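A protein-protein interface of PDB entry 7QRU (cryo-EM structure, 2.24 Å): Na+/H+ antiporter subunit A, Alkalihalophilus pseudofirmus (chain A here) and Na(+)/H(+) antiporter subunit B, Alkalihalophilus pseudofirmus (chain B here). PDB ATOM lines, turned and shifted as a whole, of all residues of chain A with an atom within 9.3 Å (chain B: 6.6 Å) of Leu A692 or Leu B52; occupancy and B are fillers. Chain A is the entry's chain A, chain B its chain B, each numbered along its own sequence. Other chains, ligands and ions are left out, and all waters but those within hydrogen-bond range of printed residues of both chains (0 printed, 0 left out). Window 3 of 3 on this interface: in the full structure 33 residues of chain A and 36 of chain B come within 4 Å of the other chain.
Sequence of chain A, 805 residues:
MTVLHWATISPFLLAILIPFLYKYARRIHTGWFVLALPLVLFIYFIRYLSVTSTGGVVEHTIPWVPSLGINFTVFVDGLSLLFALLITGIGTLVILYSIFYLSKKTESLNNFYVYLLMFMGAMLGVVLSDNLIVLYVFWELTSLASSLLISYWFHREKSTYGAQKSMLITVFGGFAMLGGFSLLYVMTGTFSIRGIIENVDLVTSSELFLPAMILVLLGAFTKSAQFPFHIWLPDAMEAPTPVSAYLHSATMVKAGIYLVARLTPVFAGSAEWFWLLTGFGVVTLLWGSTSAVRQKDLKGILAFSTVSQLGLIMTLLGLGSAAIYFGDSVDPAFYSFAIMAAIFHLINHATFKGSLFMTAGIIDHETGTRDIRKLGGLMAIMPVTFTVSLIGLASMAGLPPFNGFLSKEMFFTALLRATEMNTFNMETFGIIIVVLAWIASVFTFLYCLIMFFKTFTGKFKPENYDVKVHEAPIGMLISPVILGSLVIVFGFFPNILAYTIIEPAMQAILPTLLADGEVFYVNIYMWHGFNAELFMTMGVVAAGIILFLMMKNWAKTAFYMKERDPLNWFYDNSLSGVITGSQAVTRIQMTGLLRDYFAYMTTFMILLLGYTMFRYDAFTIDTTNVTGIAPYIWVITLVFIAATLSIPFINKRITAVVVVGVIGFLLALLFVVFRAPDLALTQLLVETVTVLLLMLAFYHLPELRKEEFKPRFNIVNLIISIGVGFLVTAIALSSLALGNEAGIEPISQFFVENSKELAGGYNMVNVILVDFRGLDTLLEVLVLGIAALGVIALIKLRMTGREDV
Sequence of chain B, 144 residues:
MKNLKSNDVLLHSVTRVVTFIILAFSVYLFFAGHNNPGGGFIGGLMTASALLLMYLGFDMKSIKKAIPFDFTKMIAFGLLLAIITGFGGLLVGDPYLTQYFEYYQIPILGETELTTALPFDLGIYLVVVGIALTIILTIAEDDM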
ATOM      1  N   VAL A 657     -18.051 -10.150  13.647  1.00  0.00           N
ATOM      2  CA  VAL A 657     -18.495  -8.760  13.685  1.00  0.00           C
ATOM      3  C   VAL A 657     -19.933  -8.670  13.138  1.00  0.00           C
ATOM      4  O   VAL A 657     -20.763  -7.941  13.649  1.00  0.00           O
ATOM      5  CB  VAL A 657     -17.508  -7.846  12.910  1.00  0.00           C
ATOM      6  CG1 VAL A 657     -18.150  -6.550  12.462  1.00  0.00           C
ATOM      7  CG2 VAL A 657     -16.346  -7.497  13.777  1.00  0.00           C
ATOM      8  N   LEU A 685     -26.302   3.797  17.586  1.00  0.00           N
ATOM      9  CA  LEU A 685     -25.134   4.612  17.343  1.00  0.00           C
ATOM     10  C   LEU A 685     -23.909   4.000  17.999  1.00  0.00           C
ATOM     11  O   LEU A 685     -22.887   3.910  17.401  1.00  0.00           O
ATOM     12  CB  LEU A 685     -25.374   6.027  17.873  1.00  0.00           C
ATOM     13  CG  LEU A 685     -26.401   6.799  17.028  1.00  0.00           C
ATOM     14  CD1 LEU A 685     -26.974   7.918  17.845  1.00  0.00           C
ATOM     15  CD2 LEU A 685     -25.804   7.320  15.710  1.00  0.00           C
ATOM     16  N   VAL A 686     -23.978   3.533  19.200  1.00  0.00           N
ATOM     17  CA  VAL A 686     -22.840   2.863  19.803  1.00  0.00           C
ATOM     18  C   VAL A 686     -22.486   1.598  18.996  1.00  0.00           C
ATOM     19  O   VAL A 686     -21.302   1.451  18.701  1.00  0.00           O
ATOM     20  CB  VAL A 686     -23.101   2.616  21.312  1.00  0.00           C
ATOM     21  CG1 VAL A 686     -22.175   1.588  21.887  1.00  0.00           C
ATOM     22  CG2 VAL A 686     -22.945   3.910  22.068  1.00  0.00           C
ATOM     23  N   GLU A 687     -23.467   0.776  18.595  1.00  0.00           N
ATOM     24  CA  GLU A 687     -23.162  -0.424  17.833  1.00  0.00           C
ATOM     25  C   GLU A 687     -22.419  -0.102  16.525  1.00  0.00           C
ATOM     26  O   GLU A 687     -21.434  -0.780  16.188  1.00  0.00           O
ATOM     27  CB  GLU A 687     -24.442  -1.233  17.616  1.00  0.00           C
ATOM     28  CG  GLU A 687     -24.812  -2.054  18.857  1.00  0.00           C
ATOM     29  CD  GLU A 687     -23.673  -2.249  19.862  1.00  0.00           C
ATOM     30  OE1 GLU A 687     -23.520  -1.375  20.754  1.00  0.00           O
ATOM     31  OE2 GLU A 687     -22.916  -3.272  19.768  1.00  0.00           O
ATOM     32  N   THR A 688     -22.784   0.996  15.855  1.00  0.00           N
ATOM     33  CA  THR A 688     -22.138   1.377  14.626  1.00  0.00           C
ATOM     34  C   THR A 688     -20.685   1.764  14.880  1.00  0.00           C
ATOM     35  O   THR A 688     -19.822   1.359  14.132  1.00  0.00           O
ATOM     36  CB  THR A 688     -23.008   2.412  13.879  1.00  0.00           C
ATOM     37  OG1 THR A 688     -24.024   1.555  13.326  1.00  0.00           O
ATOM     38  CG2 THR A 688     -22.280   3.230  12.839  1.00  0.00           C
ATOM     39  N   VAL A 689     -20.415   2.568  15.888  1.00  0.00           N
ATOM     40  CA  VAL A 689     -19.067   3.024  16.102  1.00  0.00           C
ATOM     41  C   VAL A 689     -18.305   1.792  16.594  1.00  0.00           C
ATOM     42  O   VAL A 689     -17.135   1.660  16.314  1.00  0.00           O
ATOM     43  CB  VAL A 689     -19.051   4.240  17.064  1.00  0.00           C
ATOM     44  CG1 VAL A 689     -17.677   4.777  17.286  1.00  0.00           C
ATOM     45  CG2 VAL A 689     -19.845   5.368  16.503  1.00  0.00           C
ATOM     46  N   THR A 690     -18.917   0.881  17.330  1.00  0.00           N
ATOM     47  CA  THR A 690     -18.188  -0.319  17.722  1.00  0.00           C
ATOM     48  C   THR A 690     -17.794  -1.258  16.578  1.00  0.00           C
ATOM     49  O   THR A 690     -16.711  -1.812  16.631  1.00  0.00           O
ATOM     50  CB  THR A 690     -18.935  -1.115  18.756  1.00  0.00           C
ATOM     51  OG1 THR A 690     -19.218  -0.099  19.725  1.00  0.00           O
ATOM     52  CG2 THR A 690     -18.100  -2.268  19.272  1.00  0.00           C
ATOM     53  N   VAL A 691     -18.456  -1.161  15.456  1.00  0.00           N
ATOM     54  CA  VAL A 691     -18.182  -1.991  14.313  1.00  0.00           C
ATOM     55  C   VAL A 691     -17.044  -1.338  13.545  1.00  0.00           C
ATOM     56  O   VAL A 691     -16.147  -2.076  13.140  1.00  0.00           O
ATOM     57  CB  VAL A 691     -19.465  -2.232  13.450  1.00  0.00           C
ATOM     58  CG1 VAL A 691     -19.219  -2.459  11.960  1.00  0.00           C
ATOM     59  CG2 VAL A 691     -20.243  -3.409  14.017  1.00  0.00           C
ATOM     60  N   LEU A 692     -17.016  -0.007  13.431  1.00  0.00           N
ATOM     61  CA  LEU A 692     -15.846   0.625  12.846  1.00  0.00           C
ATOM     62  C   LEU A 692     -14.607   0.339  13.703  1.00  0.00           C
ATOM     63  O   LEU A 692     -13.548   0.110  13.195  1.00  0.00           O
ATOM     64  CB  LEU A 692     -16.037   2.119  12.761  1.00  0.00           C
ATOM     65  CG  LEU A 692     -17.035   2.606  11.745  1.00  0.00           C
ATOM     66  CD1 LEU A 692     -17.208   4.121  11.944  1.00  0.00           C
ATOM     67  CD2 LEU A 692     -16.532   2.279  10.351  1.00  0.00           C
ATOM     68  N   LEU A 693     -14.731   0.379  15.009  1.00  0.00           N
ATOM     69  CA  LEU A 693     -13.621   0.183  15.881  1.00  0.00           C
ATOM     70  C   LEU A 693     -13.099  -1.216  15.767  1.00  0.00           C
ATOM     71  O   LEU A 693     -11.891  -1.324  15.800  1.00  0.00           O
ATOM     72  CB  LEU A 693     -14.065   0.303  17.329  1.00  0.00           C
ATOM     73  CG  LEU A 693     -13.710   1.594  18.003  1.00  0.00           C
ATOM     74  CD1 LEU A 693     -14.392   1.559  19.349  1.00  0.00           C
ATOM     75  CD2 LEU A 693     -12.213   1.680  18.157  1.00  0.00           C
ATOM     76  N   LEU A 694     -13.966  -2.250  15.786  1.00  0.00           N
ATOM     77  CA  LEU A 694     -13.544  -3.651  15.617  1.00  0.00           C
ATOM     78  C   LEU A 694     -12.809  -3.825  14.302  1.00  0.00           C
ATOM     79  O   LEU A 694     -11.713  -4.352  14.314  1.00  0.00           O
ATOM     80  CB  LEU A 694     -14.705  -4.615  15.703  1.00  0.00           C
ATOM     81  CG  LEU A 694     -15.082  -4.856  17.156  1.00  0.00           C
ATOM     82  CD1 LEU A 694     -16.510  -5.278  17.247  1.00  0.00           C
ATOM     83  CD2 LEU A 694     -14.202  -5.939  17.727  1.00  0.00           C
ATOM     84  N   MET A 695     -13.242  -3.169  13.258  1.00  0.00           N
ATOM     85  CA  MET A 695     -12.495  -3.256  12.020  1.00  0.00           C
ATOM     86  C   MET A 695     -11.194  -2.461  12.018  1.00  0.00           C
ATOM     87  O   MET A 695     -10.273  -2.854  11.342  1.00  0.00           O
ATOM     88  CB  MET A 695     -13.397  -2.805  10.861  1.00  0.00           C
ATOM     89  CG  MET A 695     -14.366  -4.033  10.540  1.00  0.00           C
ATOM     90  SD  MET A 695     -15.248  -3.413   9.195  1.00  0.00           S
ATOM     91  CE  MET A 695     -16.257  -2.177   9.989  1.00  0.00           C
ATOM     92  N   LEU A 696     -11.116  -1.321  12.665  1.00  0.00           N
ATOM     93  CA  LEU A 696      -9.862  -0.616  12.843  1.00  0.00           C
ATOM     94  C   LEU A 696      -8.915  -1.460  13.700  1.00  0.00           C
ATOM     95  O   LEU A 696      -7.754  -1.546  13.434  1.00  0.00           O
ATOM     96  CB  LEU A 696     -10.160   0.692  13.516  1.00  0.00           C
ATOM     97  CG  LEU A 696     -10.761   1.688  12.566  1.00  0.00           C
ATOM     98  CD1 LEU A 696     -11.024   2.972  13.305  1.00  0.00           C
ATOM     99  CD2 LEU A 696      -9.816   1.887  11.429  1.00  0.00           C
ATOM    100  N   ALA A 697      -9.419  -2.172  14.665  1.00  0.00           N
ATOM    101  CA  ALA A 697      -8.577  -3.069  15.416  1.00  0.00           C
ATOM    102  C   ALA A 697      -8.186  -4.293  14.592  1.00  0.00           C
ATOM    103  O   ALA A 697      -7.182  -4.884  14.936  1.00  0.00           O
ATOM    104  CB  ALA A 697      -9.279  -3.481  16.700  1.00  0.00           C
ATOM    105  N   PHE A 698      -8.968  -4.720  13.581  1.00  0.00           N
ATOM    106  CA  PHE A 698      -8.698  -5.974  12.844  1.00  0.00           C
ATOM    107  C   PHE A 698      -7.536  -5.800  11.891  1.00  0.00           C
ATOM    108  O   PHE A 698      -7.023  -6.769  11.362  1.00  0.00           O
ATOM    109  CB  PHE A 698      -9.847  -6.483  11.939  1.00  0.00           C
ATOM    110  CG  PHE A 698     -10.925  -7.158  12.749  1.00  0.00           C
ATOM    111  CD1 PHE A 698     -10.802  -7.287  14.142  1.00  0.00           C
ATOM    112  CD2 PHE A 698     -12.120  -7.504  12.154  1.00  0.00           C
ATOM    113  CE1 PHE A 698     -11.814  -7.865  14.893  1.00  0.00           C
ATOM    114  CE2 PHE A 698     -13.109  -8.106  12.913  1.00  0.00           C
ATOM    115  CZ  PHE A 698     -12.955  -8.281  14.277  1.00  0.00           C
ATOM    116  N   TYR A 699      -7.181  -4.528  11.614  1.00  0.00           N
ATOM    117  CA  TYR A 699      -5.992  -4.295  10.835  1.00  0.00           C
ATOM    118  C   TYR A 699      -4.720  -4.710  11.625  1.00  0.00           C
ATOM    119  O   TYR A 699      -3.655  -4.913  11.045  1.00  0.00           O
ATOM    120  CB  TYR A 699      -6.015  -2.851  10.356  1.00  0.00           C
ATOM    121  CG  TYR A 699      -4.714  -2.418   9.706  1.00  0.00           C
ATOM    122  CD1 TYR A 699      -3.707  -1.716  10.379  1.00  0.00           C
ATOM    123  CD2 TYR A 699      -4.495  -2.728   8.385  1.00  0.00           C
ATOM    124  CE1 TYR A 699      -2.518  -1.365   9.756  1.00  0.00           C
ATOM    125  CE2 TYR A 699      -3.323  -2.362   7.747  1.00  0.00           C
ATOM    126  CZ  TYR A 699      -2.325  -1.690   8.430  1.00  0.00           C
ATOM    127  OH  TYR A 699      -1.148  -1.317   7.834  1.00  0.00           O
ATOM    128  N   LEU B  45     -23.052  11.579  18.946  1.00  0.00           N
ATOM    129  CA  LEU B  45     -22.730  10.390  18.188  1.00  0.00           C
ATOM    130  C   LEU B  45     -23.229  10.529  16.758  1.00  0.00           C
ATOM    131  O   LEU B  45     -22.516  10.179  15.832  1.00  0.00           O
ATOM    132  CB  LEU B  45     -23.411   9.230  18.831  1.00  0.00           C
ATOM    133  CG  LEU B  45     -22.752   8.764  20.121  1.00  0.00           C
ATOM    134  CD1 LEU B  45     -23.657   7.790  20.830  1.00  0.00           C
ATOM    135  CD2 LEU B  45     -21.449   8.139  19.806  1.00  0.00           C
ATOM    136  N   THR B  47     -23.509  13.312  15.025  1.00  0.00           N
ATOM    137  CA  THR B  47     -22.566  14.195  14.346  1.00  0.00           C
ATOM    138  C   THR B  47     -21.256  13.510  14.040  1.00  0.00           C
ATOM    139  O   THR B  47     -20.752  13.562  12.937  1.00  0.00           O
ATOM    140  CB  THR B  47     -22.226  15.417  15.204  1.00  0.00           C
ATOM    141  OG1 THR B  47     -23.426  16.144  15.516  1.00  0.00           O
ATOM    142  CG2 THR B  47     -21.181  16.301  14.557  1.00  0.00           C
ATOM    143  N   ALA B  48     -20.757  12.728  14.995  1.00  0.00           N
ATOM    144  CA  ALA B  48     -19.559  11.933  14.751  1.00  0.00           C
ATOM    145  C   ALA B  48     -19.751  11.001  13.571  1.00  0.00           C
ATOM    146  O   ALA B  48     -18.893  10.890  12.741  1.00  0.00           O
ATOM    147  CB  ALA B  48     -19.209  11.162  15.994  1.00  0.00           C
ATOM    148  N   SER B  49     -20.883  10.309  13.501  1.00  0.00           N
ATOM    149  CA  SER B  49     -21.227   9.450  12.352  1.00  0.00           C
ATOM    150  C   SER B  49     -21.166  10.213  11.045  1.00  0.00           C
ATOM    151  O   SER B  49     -20.669   9.659  10.083  1.00  0.00           O
ATOM    152  CB  SER B  49     -22.597   8.875  12.512  1.00  0.00           C
ATOM    153  OG  SER B  49     -22.667   8.220  13.785  1.00  0.00           O
ATOM    154  N   ALA B  50     -21.695  11.461  10.992  1.00  0.00           N
ATOM    155  CA  ALA B  50     -21.513  12.239   9.771  1.00  0.00           C
ATOM    156  C   ALA B  50     -20.031  12.485   9.443  1.00  0.00           C
ATOM    157  O   ALA B  50     -19.624  12.458   8.297  1.00  0.00           O
ATOM    158  CB  ALA B  50     -22.270  13.518   9.837  1.00  0.00           C
ATOM    159  N   LEU B  51     -19.189  12.817  10.405  1.00  0.00           N
ATOM    160  CA  LEU B  51     -17.808  13.071  10.034  1.00  0.00           C
ATOM    161  C   LEU B  51     -17.162  11.757   9.680  1.00  0.00           C
ATOM    162  O   LEU B  51     -16.439  11.716   8.719  1.00  0.00           O
ATOM    163  CB  LEU B  51     -17.023  13.819  11.115  1.00  0.00           C
ATOM    164  CG  LEU B  51     -17.713  15.051  11.672  1.00  0.00           C
ATOM    165  CD1 LEU B  51     -16.904  15.652  12.766  1.00  0.00           C
ATOM    166  CD2 LEU B  51     -18.037  16.100  10.605  1.00  0.00           C
ATOM    167  N   LEU B  52     -17.469  10.659  10.338  1.00  0.00           N
ATOM    168  CA  LEU B  52     -16.883   9.383   9.975  1.00  0.00           C
ATOM    169  C   LEU B  52     -17.286   9.019   8.563  1.00  0.00           C
ATOM    170  O   LEU B  52     -16.429   8.491   7.843  1.00  0.00           O
ATOM    171  CB  LEU B  52     -17.334   8.307  10.976  1.00  0.00           C
ATOM    172  CG  LEU B  52     -16.759   8.587  12.379  1.00  0.00           C
ATOM    173  CD1 LEU B  52     -17.403   7.701  13.472  1.00  0.00           C
ATOM    174  CD2 LEU B  52     -15.234   8.465  12.353  1.00  0.00           C
ATOM    175  N   LEU B  53     -18.583   9.203   8.174  1.00  0.00           N
ATOM    176  CA  LEU B  53     -18.940   8.840   6.816  1.00  0.00           C
ATOM    177  C   LEU B  53     -18.110   9.618   5.777  1.00  0.00           C
ATOM    178  O   LEU B  53     -17.674   8.994   4.816  1.00  0.00           O
ATOM    179  CB  LEU B  53     -20.422   9.064   6.660  1.00  0.00           C
ATOM    180  CG  LEU B  53     -20.912   8.866   5.228  1.00  0.00           C
ATOM    181  CD1 LEU B  53     -20.619   7.446   4.779  1.00  0.00           C
ATOM    182  CD2 LEU B  53     -22.377   9.183   5.183  1.00  0.00           C
ATOM    183  N   MET B  54     -17.765  10.908   6.024  1.00  0.00           N
ATOM    184  CA  MET B  54     -16.846  11.674   5.193  1.00  0.00           C
ATOM    185  C   MET B  54     -15.479  11.000   5.138  1.00  0.00           C
ATOM    186  O   MET B  54     -14.977  10.784   4.113  1.00  0.00           O
ATOM    187  CB  MET B  54     -16.655  13.111   5.725  1.00  0.00           C
ATOM    188  CG  MET B  54     -17.804  14.013   5.491  1.00  0.00           C
ATOM    189  SD  MET B  54     -17.760  15.544   6.517  1.00  0.00           S
ATOM    190  CE  MET B  54     -16.594  16.492   5.563  1.00  0.00           C
ATOM    191  N   TYR B  55     -14.902  10.536   6.242  1.00  0.00           N
ATOM    192  CA  TYR B  55     -13.623   9.797   6.239  1.00  0.00           C
ATOM    193  C   TYR B  55     -13.747   8.475   5.483  1.00  0.00           C
ATOM    194  O   TYR B  55     -12.997   8.183   4.570  1.00  0.00           O
ATOM    195  CB  TYR B  55     -13.094   9.622   7.662  1.00  0.00           C
ATOM    196  CG  TYR B  55     -12.348  10.816   8.183  1.00  0.00           C
ATOM    197  CD1 TYR B  55     -11.065  11.076   7.751  1.00  0.00           C
ATOM    198  CD2 TYR B  55     -12.920  11.688   9.110  1.00  0.00           C
ATOM    199  CE1 TYR B  55     -10.331  12.133   8.274  1.00  0.00           C
ATOM    200  CE2 TYR B  55     -12.222  12.772   9.631  1.00  0.00           C
ATOM    201  CZ  TYR B  55     -10.926  12.996   9.212  1.00  0.00           C
ATOM    202  OH  TYR B  55     -10.290  14.130   9.712  1.00  0.00           O
ATOM    203  N   LEU B  56     -14.826   7.758   5.687  1.00  0.00           N
ATOM    204  CA  LEU B  56     -15.068   6.522   4.951  1.00  0.00           C
ATOM    205  C   LEU B  56     -15.194   6.721   3.446  1.00  0.00           C
ATOM    206  O   LEU B  56     -14.897   5.841   2.691  1.00  0.00           O
ATOM    207  CB  LEU B  56     -16.409   6.032   5.477  1.00  0.00           C
ATOM    208  CG  LEU B  56     -16.565   4.566   5.755  1.00  0.00           C
ATOM    209  CD1 LEU B  56     -15.422   4.067   6.558  1.00  0.00           C
ATOM    210  CD2 LEU B  56     -17.863   4.372   6.530  1.00  0.00           C
ATOM    211  N   GLY B  57     -15.962   7.749   3.056  1.00  0.00           N
ATOM    212  CA  GLY B  57     -16.283   7.990   1.680  1.00  0.00           C
ATOM    213  C   GLY B  57     -15.105   8.557   0.903  1.00  0.00           C
ATOM    214  O   GLY B  57     -15.124   8.453  -0.325  1.00  0.00           O
ATOM    215  N   ILE B  67     -12.141  19.567   7.231  1.00  0.00           N
ATOM    216  CA  ILE B  67     -12.741  19.713   8.544  1.00  0.00           C
ATOM    217  C   ILE B  67     -11.610  19.581   9.558  1.00  0.00           C
ATOM    218  O   ILE B  67     -11.380  18.553  10.220  1.00  0.00           O
ATOM    219  CB  ILE B  67     -13.884  18.720   8.847  1.00  0.00           C
ATOM    220  CG1 ILE B  67     -13.418  17.270   8.745  1.00  0.00           C
ATOM    221  CG2 ILE B  67     -15.100  18.949   7.958  1.00  0.00           C
ATOM    222  CD1 ILE B  67     -14.367  16.242   9.370  1.00  0.00           C
ATOM    223  N   ALA B 132     -15.168  10.607  20.034  1.00  0.00           N
ATOM    224  CA  ALA B 132     -15.390   9.633  18.961  1.00  0.00           C
ATOM    225  C   ALA B 132     -14.379   9.824  17.852  1.00  0.00           C
ATOM    226  O   ALA B 132     -13.746   8.876  17.413  1.00  0.00           O
ATOM    227  CB  ALA B 132     -16.706   9.794  18.400  1.00  0.00           C
ATOM    228  N   LEU B 133     -14.104  11.056  17.529  1.00  0.00           N
ATOM    229  CA  LEU B 133     -13.190  11.302  16.446  1.00  0.00           C
ATOM    230  C   LEU B 133     -11.776  11.074  16.932  1.00  0.00           C
ATOM    231  O   LEU B 133     -11.005  10.547  16.180  1.00  0.00           O
ATOM    232  CB  LEU B 133     -13.386  12.742  15.949  1.00  0.00           C
ATOM    233  CG  LEU B 133     -14.384  12.893  14.800  1.00  0.00           C
ATOM    234  CD1 LEU B 133     -13.937  12.095  13.598  1.00  0.00           C
ATOM    235  CD2 LEU B 133     -15.725  12.378  15.162  1.00  0.00           C
ATOM    236  N   ILE B 136     -11.279   7.221  16.968  1.00  0.00           N
ATOM    237  CA  ILE B 136     -11.240   6.524  15.688  1.00  0.00           C
ATOM    238  C   ILE B 136     -10.090   7.000  14.824  1.00  0.00           C
ATOM    239  O   ILE B 136      -9.365   6.168  14.287  1.00  0.00           O
ATOM    240  CB  ILE B 136     -12.588   6.660  14.969  1.00  0.00           C
ATOM    241  CG1 ILE B 136     -13.539   5.653  15.610  1.00  0.00           C
ATOM    242  CG2 ILE B 136     -12.455   6.418  13.472  1.00  0.00           C
ATOM    243  CD1 ILE B 136     -14.846   6.148  15.607  1.00  0.00           C
ATOM    244  N   LEU B 137      -9.794   8.296  14.863  1.00  0.00           N
ATOM    245  CA  LEU B 137      -8.723   8.789  14.035  1.00  0.00           C
ATOM    246  C   LEU B 137      -7.349   8.409  14.566  1.00  0.00           C
ATOM    247  O   LEU B 137      -6.418   8.396  13.810  1.00  0.00           O
ATOM    248  CB  LEU B 137      -8.866  10.301  13.934  1.00  0.00           C
ATOM    249  CG  LEU B 137     -10.033  10.814  13.070  1.00  0.00           C
ATOM    250  CD1 LEU B 137      -9.846  12.290  12.824  1.00  0.00           C
ATOM    251  CD2 LEU B 137     -10.140  10.107  11.767  1.00  0.00           C
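Along chain B the printed residues that touch a printed residue of chain A span positions 45 to 136. Of the 16 printed residues of chain A, 4 touch a printed residue of chain B. Hydrophobic or aromatic side chains of chain A within 4 Å of the printed part of chain B: Leu A685, Val A689, Leu A692 and Leu A696. Along chain A the printed residues that touch a printed residue of chain B span positions 685 to 696. Among the printed residues, no Asp or Glu carboxylate lies within 4 Å of a Lys or Arg side-chain nitrogen of the other chain.
Of the printed residues of chain B, Leu A692 touches Leu B52. Printed residues of chain A within 4 Å of Leu B52: Leu A692 (3.9 Å). Printed residues of chain B within 4 Å of Val A689: Ile B136 (3.6 Å). Printed residues of chain B within 4 Å of Leu A696: Ile B136. Val A657 touches none of the printed residues of chain B. The nearest residue of chain B that does not touch Leu A692 is Leu B56 (4.3 Å). The nearest printed residue of chain B that does not touch Val A689 is Leu B52 (4.5 Å).
The side-chain hydroxyl (OG) of Ser B49 sits at hydrogen-bond distance from the backbone carbonyl oxygen (O) of Leu B45.
Among the printed residues, pairs that only touch across the chains: Val A689 with Ile B136, Leu A696 with Ile B136, Leu A685 with Ser B49, Leu A685 with Leu B45 and Leu A692 with Leu B52.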
